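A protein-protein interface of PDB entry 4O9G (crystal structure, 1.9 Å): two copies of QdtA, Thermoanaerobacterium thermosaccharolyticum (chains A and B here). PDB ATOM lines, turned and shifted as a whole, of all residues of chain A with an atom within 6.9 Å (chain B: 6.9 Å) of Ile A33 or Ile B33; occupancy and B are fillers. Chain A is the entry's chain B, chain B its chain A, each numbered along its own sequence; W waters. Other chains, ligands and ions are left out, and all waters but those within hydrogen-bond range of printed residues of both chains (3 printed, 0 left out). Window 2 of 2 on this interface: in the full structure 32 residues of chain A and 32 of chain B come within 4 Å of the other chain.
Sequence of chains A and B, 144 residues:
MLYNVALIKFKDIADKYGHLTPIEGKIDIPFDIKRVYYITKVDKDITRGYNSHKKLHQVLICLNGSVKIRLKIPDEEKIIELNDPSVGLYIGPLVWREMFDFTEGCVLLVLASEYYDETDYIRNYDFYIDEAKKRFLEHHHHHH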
ATOM      1  N   ILE A  23       0.363 -14.709   8.525  1.00  0.00           N
ATOM      2  CA  ILE A  23      -0.466 -14.208   7.440  1.00  0.00           C
ATOM      3  C   ILE A  23      -1.400 -13.156   7.988  1.00  0.00           C
ATOM      4  O   ILE A  23      -2.268 -13.460   8.783  1.00  0.00           O
ATOM      5  CB  ILE A  23      -1.313 -15.311   6.825  1.00  0.00           C
ATOM      6  CG1 ILE A  23      -0.432 -16.527   6.468  1.00  0.00           C
ATOM      7  CG2 ILE A  23      -2.062 -14.787   5.611  1.00  0.00           C
ATOM      8  CD1 ILE A  23      -1.200 -17.652   5.823  1.00  0.00           C
ATOM      9  N   GLU A  24      -1.210 -11.926   7.546  1.00  0.00           N
ATOM     10  CA  GLU A  24      -2.020 -10.814   7.997  1.00  0.00           C
ATOM     11  C   GLU A  24      -3.023 -10.432   6.936  1.00  0.00           C
ATOM     12  O   GLU A  24      -2.678 -10.228   5.761  1.00  0.00           O
ATOM     13  CB  GLU A  24      -1.122  -9.628   8.335  1.00  0.00           C
ATOM     14  CG  GLU A  24      -0.192  -9.910   9.504  1.00  0.00           C
ATOM     15  CD  GLU A  24       0.680  -8.725   9.825  1.00  0.00           C
ATOM     16  OE1 GLU A  24       1.300  -8.207   8.894  1.00  0.00           O
ATOM     17  OE2 GLU A  24       0.719  -8.291  10.988  1.00  0.00           O
ATOM     18  N   GLY A  25      -4.285 -10.371   7.338  1.00  0.00           N
ATOM     19  CA  GLY A  25      -5.355  -9.968   6.431  1.00  0.00           C
ATOM     20  C   GLY A  25      -5.094  -8.673   5.700  1.00  0.00           C
ATOM     21  O   GLY A  25      -4.663  -7.688   6.292  1.00  0.00           O
ATOM     22  N   LYS A  26      -5.382  -8.689   4.401  1.00  0.00           N
ATOM     23  CA  LYS A  26      -5.178  -7.558   3.491  1.00  0.00           C
ATOM     24  C   LYS A  26      -3.728  -7.263   3.172  1.00  0.00           C
ATOM     25  O   LYS A  26      -3.432  -6.493   2.266  1.00  0.00           O
ATOM     26  CB  LYS A  26      -5.875  -6.286   3.960  1.00  0.00           C
ATOM     27  CG  LYS A  26      -7.391  -6.416   4.000  1.00  0.00           C
ATOM     28  CD  LYS A  26      -8.083  -5.096   4.300  1.00  0.00           C
ATOM     29  CE  LYS A  26      -8.052  -4.740   5.785  1.00  0.00           C
ATOM     30  NZ  LYS A  26      -8.023  -3.269   6.011  1.00  0.00           N
ATOM     31  N   ILE A  29      -2.419 -11.638   2.190  1.00  0.00           N
ATOM     32  CA  ILE A  29      -3.454 -11.998   1.261  1.00  0.00           C
ATOM     33  C   ILE A  29      -4.311 -10.753   1.000  1.00  0.00           C
ATOM     34  O   ILE A  29      -4.379  -9.840   1.816  1.00  0.00           O
ATOM     35  CB  ILE A  29      -4.314 -13.155   1.805  1.00  0.00           C
ATOM     36  CG1 ILE A  29      -4.937 -12.773   3.142  1.00  0.00           C
ATOM     37  CG2 ILE A  29      -3.494 -14.426   2.012  1.00  0.00           C
ATOM     38  CD1 ILE A  29      -5.935 -13.798   3.605  1.00  0.00           C
ATOM     39  N   PHE A  31      -7.469 -10.111   1.050  1.00  0.00           N
ATOM     40  CA  PHE A  31      -8.743  -9.858   1.717  1.00  0.00           C
ATOM     41  C   PHE A  31      -8.649 -10.046   3.235  1.00  0.00           C
ATOM     42  O   PHE A  31      -7.655 -10.557   3.735  1.00  0.00           O
ATOM     43  CB  PHE A  31      -9.800 -10.769   1.113  1.00  0.00           C
ATOM     44  CG  PHE A  31      -9.446 -12.226   1.191  1.00  0.00           C
ATOM     45  CD1 PHE A  31      -9.635 -12.923   2.356  1.00  0.00           C
ATOM     46  CD2 PHE A  31      -8.934 -12.890   0.090  1.00  0.00           C
ATOM     47  CE1 PHE A  31      -9.332 -14.274   2.431  1.00  0.00           C
ATOM     48  CE2 PHE A  31      -8.618 -14.247   0.149  1.00  0.00           C
ATOM     49  CZ  PHE A  31      -8.810 -14.941   1.323  1.00  0.00           C
ATOM     50  N   ASP A  32      -9.667  -9.582   3.946  1.00  0.00           N
ATOM     51  CA  ASP A  32      -9.799  -9.758   5.396  1.00  0.00           C
ATOM     52  C   ASP A  32     -10.256 -11.167   5.693  1.00  0.00           C
ATOM     53  O   ASP A  32     -11.136 -11.695   5.009  1.00  0.00           O
ATOM     54  CB  ASP A  32     -10.864  -8.825   5.970  1.00  0.00           C
ATOM     55  CG  ASP A  32     -10.370  -7.390   6.144  1.00  0.00           C
ATOM     56  OD1 ASP A  32      -9.312  -7.181   6.754  1.00  0.00           O
ATOM     57  OD2 ASP A  32     -11.062  -6.474   5.680  1.00  0.00           O
ATOM     58  N   ILE A  33      -9.660 -11.765   6.709  1.00  0.00           N
ATOM     59  CA  ILE A  33     -10.032 -13.132   7.133  1.00  0.00           C
ATOM     60  C   ILE A  33     -11.234 -13.093   8.065  1.00  0.00           C
ATOM     61  O   ILE A  33     -11.113 -12.813   9.269  1.00  0.00           O
ATOM     62  CB  ILE A  33      -8.868 -13.840   7.852  1.00  0.00           C
ATOM     63  CG1 ILE A  33      -7.614 -13.809   6.993  1.00  0.00           C
ATOM     64  CG2 ILE A  33      -9.221 -15.302   8.166  1.00  0.00           C
ATOM     65  CD1 ILE A  33      -6.333 -13.944   7.802  1.00  0.00           C
ATOM     66  N   LYS A  34     -12.397 -13.397   7.512  1.00  0.00           N
ATOM     67  CA  LYS A  34     -13.611 -13.507   8.288  1.00  0.00           C
ATOM     68  C   LYS A  34     -13.812 -14.899   8.881  1.00  0.00           C
ATOM     69  O   LYS A  34     -14.537 -15.088   9.863  1.00  0.00           O
ATOM     70  CB  LYS A  34     -14.793 -13.130   7.391  1.00  0.00           C
ATOM     71  CG  LYS A  34     -14.827 -11.644   7.065  1.00  0.00           C
ATOM     72  CD  LYS A  34     -16.126 -11.251   6.376  1.00  0.00           C
ATOM     73  CE  LYS A  34     -16.336  -9.742   6.336  1.00  0.00           C
ATOM     74  NZ  LYS A  34     -15.204  -9.024   5.687  1.00  0.00           N
ATOM     75  N   ARG A  35     -13.170 -15.879   8.271  1.00  0.00           N
ATOM     76  CA  ARG A  35     -13.453 -17.257   8.579  1.00  0.00           C
ATOM     77  C   ARG A  35     -12.247 -18.089   8.156  1.00  0.00           C
ATOM     78  O   ARG A  35     -11.621 -17.829   7.125  1.00  0.00           O
ATOM     79  CB  ARG A  35     -14.707 -17.733   7.836  1.00  0.00           C
ATOM     80  CG  ARG A  35     -14.868 -19.241   7.944  1.00  0.00           C
ATOM     81  CD  ARG A  35     -16.095 -19.764   7.229  1.00  0.00           C
ATOM     82  NE  ARG A  35     -16.328 -19.141   5.939  1.00  0.00           N
ATOM     83  CZ  ARG A  35     -16.527 -19.810   4.813  1.00  0.00           C
ATOM     84  NH1 ARG A  35     -16.751 -19.148   3.692  1.00  0.00           N
ATOM     85  NH2 ARG A  35     -16.480 -21.141   4.801  1.00  0.00           N
ATOM     86  N   VAL A  36     -11.900 -19.053   8.986  1.00  0.00           N
ATOM     87  CA  VAL A  36     -10.946 -20.071   8.599  1.00  0.00           C
ATOM     88  C   VAL A  36     -11.638 -21.423   8.759  1.00  0.00           C
ATOM     89  O   VAL A  36     -12.643 -21.557   9.439  1.00  0.00           O
ATOM     90  CB  VAL A  36      -9.621 -20.039   9.418  1.00  0.00           C
ATOM     91  CG1 VAL A  36      -8.913 -18.700   9.330  1.00  0.00           C
ATOM     92  CG2 VAL A  36      -9.833 -20.390  10.876  1.00  0.00           C
ATOM     93  N   VAL A 110      -7.892 -23.398   5.324  1.00  0.00           N
ATOM     94  CA  VAL A 110      -8.464 -22.470   4.381  1.00  0.00           C
ATOM     95  C   VAL A 110      -8.768 -21.124   5.040  1.00  0.00           C
ATOM     96  O   VAL A 110      -9.399 -21.068   6.100  1.00  0.00           O
ATOM     97  CB  VAL A 110      -9.729 -23.040   3.711  1.00  0.00           C
ATOM     98  CG1 VAL A 110     -10.286 -22.048   2.702  1.00  0.00           C
ATOM     99  CG2 VAL A 110      -9.402 -24.363   2.998  1.00  0.00           C
ATOM    100  N   LEU A 111      -8.331 -20.059   4.383  1.00  0.00           N
ATOM    101  CA  LEU A 111      -8.741 -18.721   4.759  1.00  0.00           C
ATOM    102  C   LEU A 111      -9.787 -18.217   3.783  1.00  0.00           C
ATOM    103  O   LEU A 111      -9.578 -18.226   2.558  1.00  0.00           O
ATOM    104  CB  LEU A 111      -7.567 -17.756   4.793  1.00  0.00           C
ATOM    105  CG  LEU A 111      -6.262 -18.334   5.331  1.00  0.00           C
ATOM    106  CD1 LEU A 111      -5.151 -17.322   5.151  1.00  0.00           C
ATOM    107  CD2 LEU A 111      -6.399 -18.700   6.788  1.00  0.00           C
ATOM    108  N   ALA A 112     -10.882 -17.752   4.345  1.00  0.00           N
ATOM    109  CA  ALA A 112     -12.043 -17.368   3.543  1.00  0.00           C
ATOM    110  C   ALA A 112     -12.435 -15.889   3.742  1.00  0.00           C
ATOM    111  O   ALA A 112     -12.387 -15.359   4.877  1.00  0.00           O
ATOM    112  CB  ALA A 112     -13.202 -18.255   3.912  1.00  0.00           C
ATOM    113  N   SER A 113     -12.890 -15.260   2.664  1.00  0.00           N
ATOM    114  CA  SER A 113     -13.248 -13.833   2.678  1.00  0.00           C
ATOM    115  C   SER A 113     -14.624 -13.528   3.214  1.00  0.00           C
ATOM    116  O   SER A 113     -14.954 -12.372   3.399  1.00  0.00           O
ATOM    117  CB  SER A 113     -13.125 -13.188   1.284  1.00  0.00           C
ATOM    118  OG  SER A 113     -14.137 -13.647   0.381  1.00  0.00           O
ATOM    119  N   GLU A 114     -15.454 -14.537   3.427  1.00  0.00           N
ATOM    120  CA  GLU A 114     -16.771 -14.304   3.955  1.00  0.00           C
ATOM    121  C   GLU A 114     -17.152 -15.409   4.902  1.00  0.00           C
ATOM    122  O   GLU A 114     -16.635 -16.533   4.843  1.00  0.00           O
ATOM    123  CB  GLU A 114     -17.805 -14.198   2.838  1.00  0.00           C
ATOM    124  CG  GLU A 114     -17.469 -13.187   1.755  1.00  0.00           C
ATOM    125  CD  GLU A 114     -17.625 -11.728   2.176  1.00  0.00           C
ATOM    126  OE1 GLU A 114     -18.213 -11.432   3.244  1.00  0.00           O
ATOM    127  OE2 GLU A 114     -17.162 -10.872   1.394  1.00  0.00           O
ATOM    128  N   ILE B  23     -14.098 -21.889  11.852  1.00  0.00           N
ATOM    129  CA  ILE B  23     -14.019 -20.898  12.906  1.00  0.00           C
ATOM    130  C   ILE B  23     -14.275 -19.567  12.255  1.00  0.00           C
ATOM    131  O   ILE B  23     -13.460 -19.099  11.464  1.00  0.00           O
ATOM    132  CB  ILE B  23     -12.639 -20.874  13.537  1.00  0.00           C
ATOM    133  CG1 ILE B  23     -12.247 -22.284  14.001  1.00  0.00           C
ATOM    134  CG2 ILE B  23     -12.608 -19.872  14.688  1.00  0.00           C
ATOM    135  CD1 ILE B  23     -10.870 -22.328  14.603  1.00  0.00           C
ATOM    136  N   GLU B  24     -15.427 -18.988  12.580  1.00  0.00           N
ATOM    137  CA  GLU B  24     -15.820 -17.683  12.094  1.00  0.00           C
ATOM    138  C   GLU B  24     -15.535 -16.595  13.149  1.00  0.00           C
ATOM    139  O   GLU B  24     -15.917 -16.724  14.329  1.00  0.00           O
ATOM    140  CB  GLU B  24     -17.299 -17.705  11.723  1.00  0.00           C
ATOM    141  CG  GLU B  24     -17.638 -18.691  10.611  1.00  0.00           C
ATOM    142  CD  GLU B  24     -19.108 -18.691  10.274  1.00  0.00           C
ATOM    143  OE1 GLU B  24     -19.887 -18.939  11.200  1.00  0.00           O
ATOM    144  OE2 GLU B  24     -19.483 -18.433   9.105  1.00  0.00           O
ATOM    145  N   GLY B  25     -14.832 -15.546  12.717  1.00  0.00           N
ATOM    146  CA  GLY B  25     -14.512 -14.411  13.586  1.00  0.00           C
ATOM    147  C   GLY B  25     -15.759 -13.886  14.252  1.00  0.00           C
ATOM    148  O   GLY B  25     -16.781 -13.706  13.587  1.00  0.00           O
ATOM    149  N   LYS B  26     -15.660 -13.708  15.569  1.00  0.00           N
ATOM    150  CA  LYS B  26     -16.690 -13.111  16.428  1.00  0.00           C
ATOM    151  C   LYS B  26     -17.824 -14.054  16.745  1.00  0.00           C
ATOM    152  O   LYS B  26     -18.683 -13.755  17.568  1.00  0.00           O
ATOM    153  CB  LYS B  26     -17.213 -11.806  15.851  1.00  0.00           C
ATOM    154  CG  LYS B  26     -16.142 -10.726  15.818  1.00  0.00           C
ATOM    155  CD  LYS B  26     -16.724  -9.365  15.473  1.00  0.00           C
ATOM    156  CE  LYS B  26     -17.151  -9.280  14.013  1.00  0.00           C
ATOM    157  NZ  LYS B  26     -18.557  -8.808  13.865  1.00  0.00           N
ATOM    158  N   ILE B  29     -15.069 -17.603  17.928  1.00  0.00           N
ATOM    159  CA  ILE B  29     -14.177 -16.970  18.856  1.00  0.00           C
ATOM    160  C   ILE B  29     -14.643 -15.538  19.026  1.00  0.00           C
ATOM    161  O   ILE B  29     -15.361 -15.035  18.207  1.00  0.00           O
ATOM    162  CB  ILE B  29     -12.745 -17.012  18.357  1.00  0.00           C
ATOM    163  CG1 ILE B  29     -12.638 -16.298  16.983  1.00  0.00           C
ATOM    164  CG2 ILE B  29     -12.302 -18.476  18.275  1.00  0.00           C
ATOM    165  CD1 ILE B  29     -11.182 -16.037  16.597  1.00  0.00           C
ATOM    166  N   PHE B  31     -13.212 -12.611  18.964  1.00  0.00           N
ATOM    167  CA  PHE B  31     -12.644 -11.495  18.230  1.00  0.00           C
ATOM    168  C   PHE B  31     -12.582 -11.720  16.732  1.00  0.00           C
ATOM    169  O   PHE B  31     -12.768 -12.833  16.239  1.00  0.00           O
ATOM    170  CB  PHE B  31     -11.260 -11.167  18.774  1.00  0.00           C
ATOM    171  CG  PHE B  31     -10.297 -12.334  18.777  1.00  0.00           C
ATOM    172  CD1 PHE B  31      -9.519 -12.594  17.677  1.00  0.00           C
ATOM    173  CD2 PHE B  31     -10.123 -13.113  19.903  1.00  0.00           C
ATOM    174  CE1 PHE B  31      -8.596 -13.624  17.691  1.00  0.00           C
ATOM    175  CE2 PHE B  31      -9.221 -14.175  19.911  1.00  0.00           C
ATOM    176  CZ  PHE B  31      -8.450 -14.422  18.792  1.00  0.00           C
ATOM    177  N   ASP B  32     -12.313 -10.647  16.018  1.00  0.00           N
ATOM    178  CA  ASP B  32     -12.098 -10.689  14.576  1.00  0.00           C
ATOM    179  C   ASP B  32     -10.696 -11.175  14.333  1.00  0.00           C
ATOM    180  O   ASP B  32      -9.759 -10.822  15.063  1.00  0.00           O
ATOM    181  CB  ASP B  32     -12.204  -9.294  13.957  1.00  0.00           C
ATOM    182  CG  ASP B  32     -13.641  -8.831  13.754  1.00  0.00           C
ATOM    183  OD1 ASP B  32     -14.477  -9.587  13.205  1.00  0.00           O
ATOM    184  OD2 ASP B  32     -13.929  -7.677  14.129  1.00  0.00           O
ATOM    185  N   ILE B  33     -10.536 -11.945  13.267  1.00  0.00           N
ATOM    186  CA  ILE B  33      -9.249 -12.517  12.951  1.00  0.00           C
ATOM    187  C   ILE B  33      -8.532 -11.550  12.026  1.00  0.00           C
ATOM    188  O   ILE B  33      -8.847 -11.488  10.817  1.00  0.00           O
ATOM    189  CB  ILE B  33      -9.380 -13.895  12.247  1.00  0.00           C
ATOM    190  CG1 ILE B  33     -10.205 -14.869  13.087  1.00  0.00           C
ATOM    191  CG2 ILE B  33      -8.001 -14.489  12.017  1.00  0.00           C
ATOM    192  CD1 ILE B  33     -10.678 -16.106  12.327  1.00  0.00           C
ATOM    193  N   LYS B  34      -7.558 -10.830  12.568  1.00  0.00           N
ATOM    194  CA  LYS B  34      -6.728  -9.909  11.783  1.00  0.00           C
ATOM    195  C   LYS B  34      -5.485 -10.584  11.206  1.00  0.00           C
ATOM    196  O   LYS B  34      -4.912 -10.139  10.167  1.00  0.00           O
ATOM    197  CB  LYS B  34      -6.360  -8.668  12.616  1.00  0.00           C
ATOM    198  CG  LYS B  34      -7.579  -7.809  12.998  1.00  0.00           C
ATOM    199  CD  LYS B  34      -7.255  -6.322  13.144  1.00  0.00           C
ATOM    200  CE  LYS B  34      -8.052  -5.648  14.265  1.00  0.00           C
ATOM    201  NZ  LYS B  34      -9.527  -5.845  14.153  1.00  0.00           N
ATOM    202  N   ARG B  35      -5.095 -11.681  11.844  1.00  0.00           N
ATOM    203  CA  ARG B  35      -3.844 -12.342  11.549  1.00  0.00           C
ATOM    204  C   ARG B  35      -3.868 -13.792  12.029  1.00  0.00           C
ATOM    205  O   ARG B  35      -4.401 -14.081  13.089  1.00  0.00           O
ATOM    206  CB  ARG B  35      -2.694 -11.594  12.204  1.00  0.00           C
ATOM    207  CG  ARG B  35      -1.438 -12.440  12.360  1.00  0.00           C
ATOM    208  CD  ARG B  35      -0.277 -11.632  12.920  1.00  0.00           C
ATOM    209  NE  ARG B  35      -0.611 -11.087  14.233  1.00  0.00           N
ATOM    210  CZ  ARG B  35       0.016 -11.402  15.362  1.00  0.00           C
ATOM    211  NH1 ARG B  35      -0.372 -10.848  16.491  1.00  0.00           N
ATOM    212  NH2 ARG B  35       1.019 -12.279  15.373  1.00  0.00           N
ATOM    213  N   VAL B  36      -3.342 -14.698  11.210  1.00  0.00           N
ATOM    214  CA  VAL B  36      -3.034 -16.027  11.667  1.00  0.00           C
ATOM    215  C   VAL B  36      -1.561 -16.296  11.540  1.00  0.00           C
ATOM    216  O   VAL B  36      -0.859 -15.655  10.762  1.00  0.00           O
ATOM    217  CB  VAL B  36      -3.822 -17.133  10.942  1.00  0.00           C
ATOM    218  CG1 VAL B  36      -5.312 -16.898  11.046  1.00  0.00           C
ATOM    219  CG2 VAL B  36      -3.359 -17.307   9.487  1.00  0.00           C
ATOM    220  N   VAL B 110      -2.398 -20.388  15.309  1.00  0.00           N
ATOM    221  CA  VAL B 110      -2.840 -19.339  16.205  1.00  0.00           C
ATOM    222  C   VAL B 110      -3.639 -18.317  15.398  1.00  0.00           C
ATOM    223  O   VAL B 110      -3.216 -17.869  14.312  1.00  0.00           O
ATOM    224  CB  VAL B 110      -1.632 -18.632  16.853  1.00  0.00           C
ATOM    225  CG1 VAL B 110      -2.081 -17.586  17.852  1.00  0.00           C
ATOM    226  CG2 VAL B 110      -0.711 -19.683  17.483  1.00  0.00           C
ATOM    227  N   LEU B 111      -4.802 -17.981  15.931  1.00  0.00           N
ATOM    228  CA  LEU B 111      -5.583 -16.877  15.436  1.00  0.00           C
ATOM    229  C   LEU B 111      -5.331 -15.678  16.346  1.00  0.00           C
ATOM    230  O   LEU B 111      -5.385 -15.812  17.575  1.00  0.00           O
ATOM    231  CB  LEU B 111      -7.062 -17.270  15.418  1.00  0.00           C
ATOM    232  CG  LEU B 111      -7.372 -18.652  14.838  1.00  0.00           C
ATOM    233  CD1 LEU B 111      -8.859 -18.987  14.952  1.00  0.00           C
ATOM    234  CD2 LEU B 111      -6.931 -18.831  13.400  1.00  0.00           C
ATOM    235  N   ALA B 112      -5.073 -14.512  15.757  1.00  0.00           N
ATOM    236  CA  ALA B 112      -4.712 -13.337  16.548  1.00  0.00           C
ATOM    237  C   ALA B 112      -5.634 -12.106  16.281  1.00  0.00           C
ATOM    238  O   ALA B 112      -6.080 -11.899  15.134  1.00  0.00           O
ATOM    239  CB  ALA B 112      -3.245 -13.008  16.311  1.00  0.00           C
ATOM    240  N   SER B 113      -5.918 -11.342  17.343  1.00  0.00           N
ATOM    241  CA  SER B 113      -6.869 -10.212  17.306  1.00  0.00           C
ATOM    242  C   SER B 113      -6.283  -8.933  16.700  1.00  0.00           C
ATOM    243  O   SER B 113      -7.010  -7.991  16.432  1.00  0.00           O
ATOM    244  CB  SER B 113      -7.434  -9.915  18.716  1.00  0.00           C
ATOM    245  OG  SER B 113      -6.428  -9.542  19.661  1.00  0.00           O
ATOM    246  N   GLU B 114      -4.976  -8.910  16.468  1.00  0.00           N
ATOM    247  CA  GLU B 114      -4.291  -7.737  15.929  1.00  0.00           C
ATOM    248  C   GLU B 114      -3.154  -8.159  15.062  1.00  0.00           C
ATOM    249  O   GLU B 114      -2.608  -9.251  15.232  1.00  0.00           O
ATOM    250  CB  GLU B 114      -3.712  -6.877  17.052  1.00  0.00           C
ATOM    251  CG  GLU B 114      -4.738  -6.435  18.060  1.00  0.00           C
ATOM    252  CD  GLU B 114      -5.688  -5.404  17.482  1.00  0.00           C
ATOM    253  OE1 GLU B 114      -5.395  -4.870  16.387  1.00  0.00           O
ATOM    254  OE2 GLU B 114      -6.705  -5.124  18.137  1.00  0.00           O
HETATM  255  O   HOH W   1     -12.668 -12.791  11.624  1.00  0.00           O
HETATM  256  O   HOH W   2     -11.170  -9.641   9.894  1.00  0.00           O
HETATM  257  O   HOH W   3      -7.887 -10.488   8.463  1.00  0.00           O
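The backbone NH (N) of Ile B23 is in hydrogen-bond range of the backbone carbonyl oxygen (O) of Val A36. The backbone NH (N) of Gly B25 lies within hydrogen-bond range of the backbone carbonyl oxygen (O) of Lys A34 (2.9 Å). O of Lys B34 sits at hydrogen-bond distance from N of Gly A25, at 2.9 Å. The backbone NH of Ile A23 lies within hydrogen-bond range of the backbone carbonyl oxygen of Val B36 (2.7 Å). The backbone carbonyl oxygen (O) of Ile B33 sits close to the backbone carbonyl oxygen (O) of Ile A33, at 3.0 Å.
The backbone NH (N) of Lys B34 lies within hydrogen-bond range of the backbone carbonyl oxygen (O) of Ala B112, at 3.1 Å. O of Arg B35 lies within hydrogen-bond range of N of Ala B112. The backbone carbonyl oxygen (O) of Glu B114 lies within hydrogen-bond range of the guanidinium group (NE) of Arg B35. N of Lys A34 lies within hydrogen-bond range of O of Ala A112, 3.3 Å away. The backbone NH (N) of Ala A112 lies within hydrogen-bond range of the backbone carbonyl oxygen (O) of Arg A35, at 2.9 Å. The guanidinium group (NE) of Arg A35 lies within hydrogen-bond range of the backbone carbonyl oxygen (O) of Glu A114, 2.8 Å away.
Arg B35 touches Ile A23. O of Lys B34 touches CA of Glu A24 (3.7 Å). Glu A24 touches Arg B35. Glu B24 touches Lys A34. CA of Arg A35 touches O of Ile B23 (3.4 Å). CD of Arg A35 touches CG of Glu B24, 3.9 Å away.
Phe A31 touches none of the printed residues of chain B. Ile A33 touches just one residue of chain B: Ile B33 (3.0 Å). Printed residues of chain B within 4 Å of Lys A34: Glu B24 and Gly B25. Of the printed residues of chain B, Val A36 touches Ile B23 (2.8 Å). Printed residues of chain A within 4 Å of Ile B23: Arg A35 (3.4 Å) and Val A36 (2.8 Å). Of the printed residues of chain A, Glu B24 touches Lys A34 (3.7 Å) and Arg A35 (3.9 Å). Ile B33 touches one residue of chain A. Printed residues of chain A within 4 Å of Val B36: Ile A23 (2.7 Å). Glu B114 touches none of the printed residues of chain A. The nearest residue of chain B that does not touch Ile A33 is Val B36 (4.5 Å). The nearest printed residue of chain A that does not touch Arg B35 is Gly A25 (4.7 Å).
Of the 16 printed residues of chain A, 7 touch a printed residue of chain B. Hydrophobic or aromatic side chains of chain B within 4 Å of the printed part of chain A: Ile B23, Ile B33 and Val B36. Among the printed residues, 11 pairs touch across the chains.
Ile A23 touches Arg B35, and with the chains exchanged Arg A35 touches Ile B23. Ile A23 touches Val B36, and with the chains exchanged Val A36 touches Ile B23. Glu A24 touches Lys B34, and with the chains exchanged Lys A34 touches Glu B24. Glu A24 touches Arg B35, and with the chains exchanged Arg A35 touches Glu B24. Positions printed for both chains: 23, 24, 25, 26, 29, 31, 32, 33, 34, 35, 36, 110, 111, 112, 113 and 114. Of the 11 pairs that touch across the chains among the printed residues, 11 have their exchanged pair printed and touching as well.
Water W3 lies within hydrogen-bond range of the backbone carbonyl oxygen (O) of Ile B33, the backbone NH (N) of Ile A33 and the backbone carbonyl oxygen (O) of Lys B34. Water W1 lies within hydrogen-bond range of the backbone NH of Ile B33 (2.8 Å), the backbone carbonyl oxygen of Ile A33 (2.8 Å) and the backbone carbonyl oxygen of Lys A34 (3.4 Å). Water W2 lies within hydrogen-bond range of O of Ile B33 (3.1 Å) and O of Ile A33 (3.2 Å).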
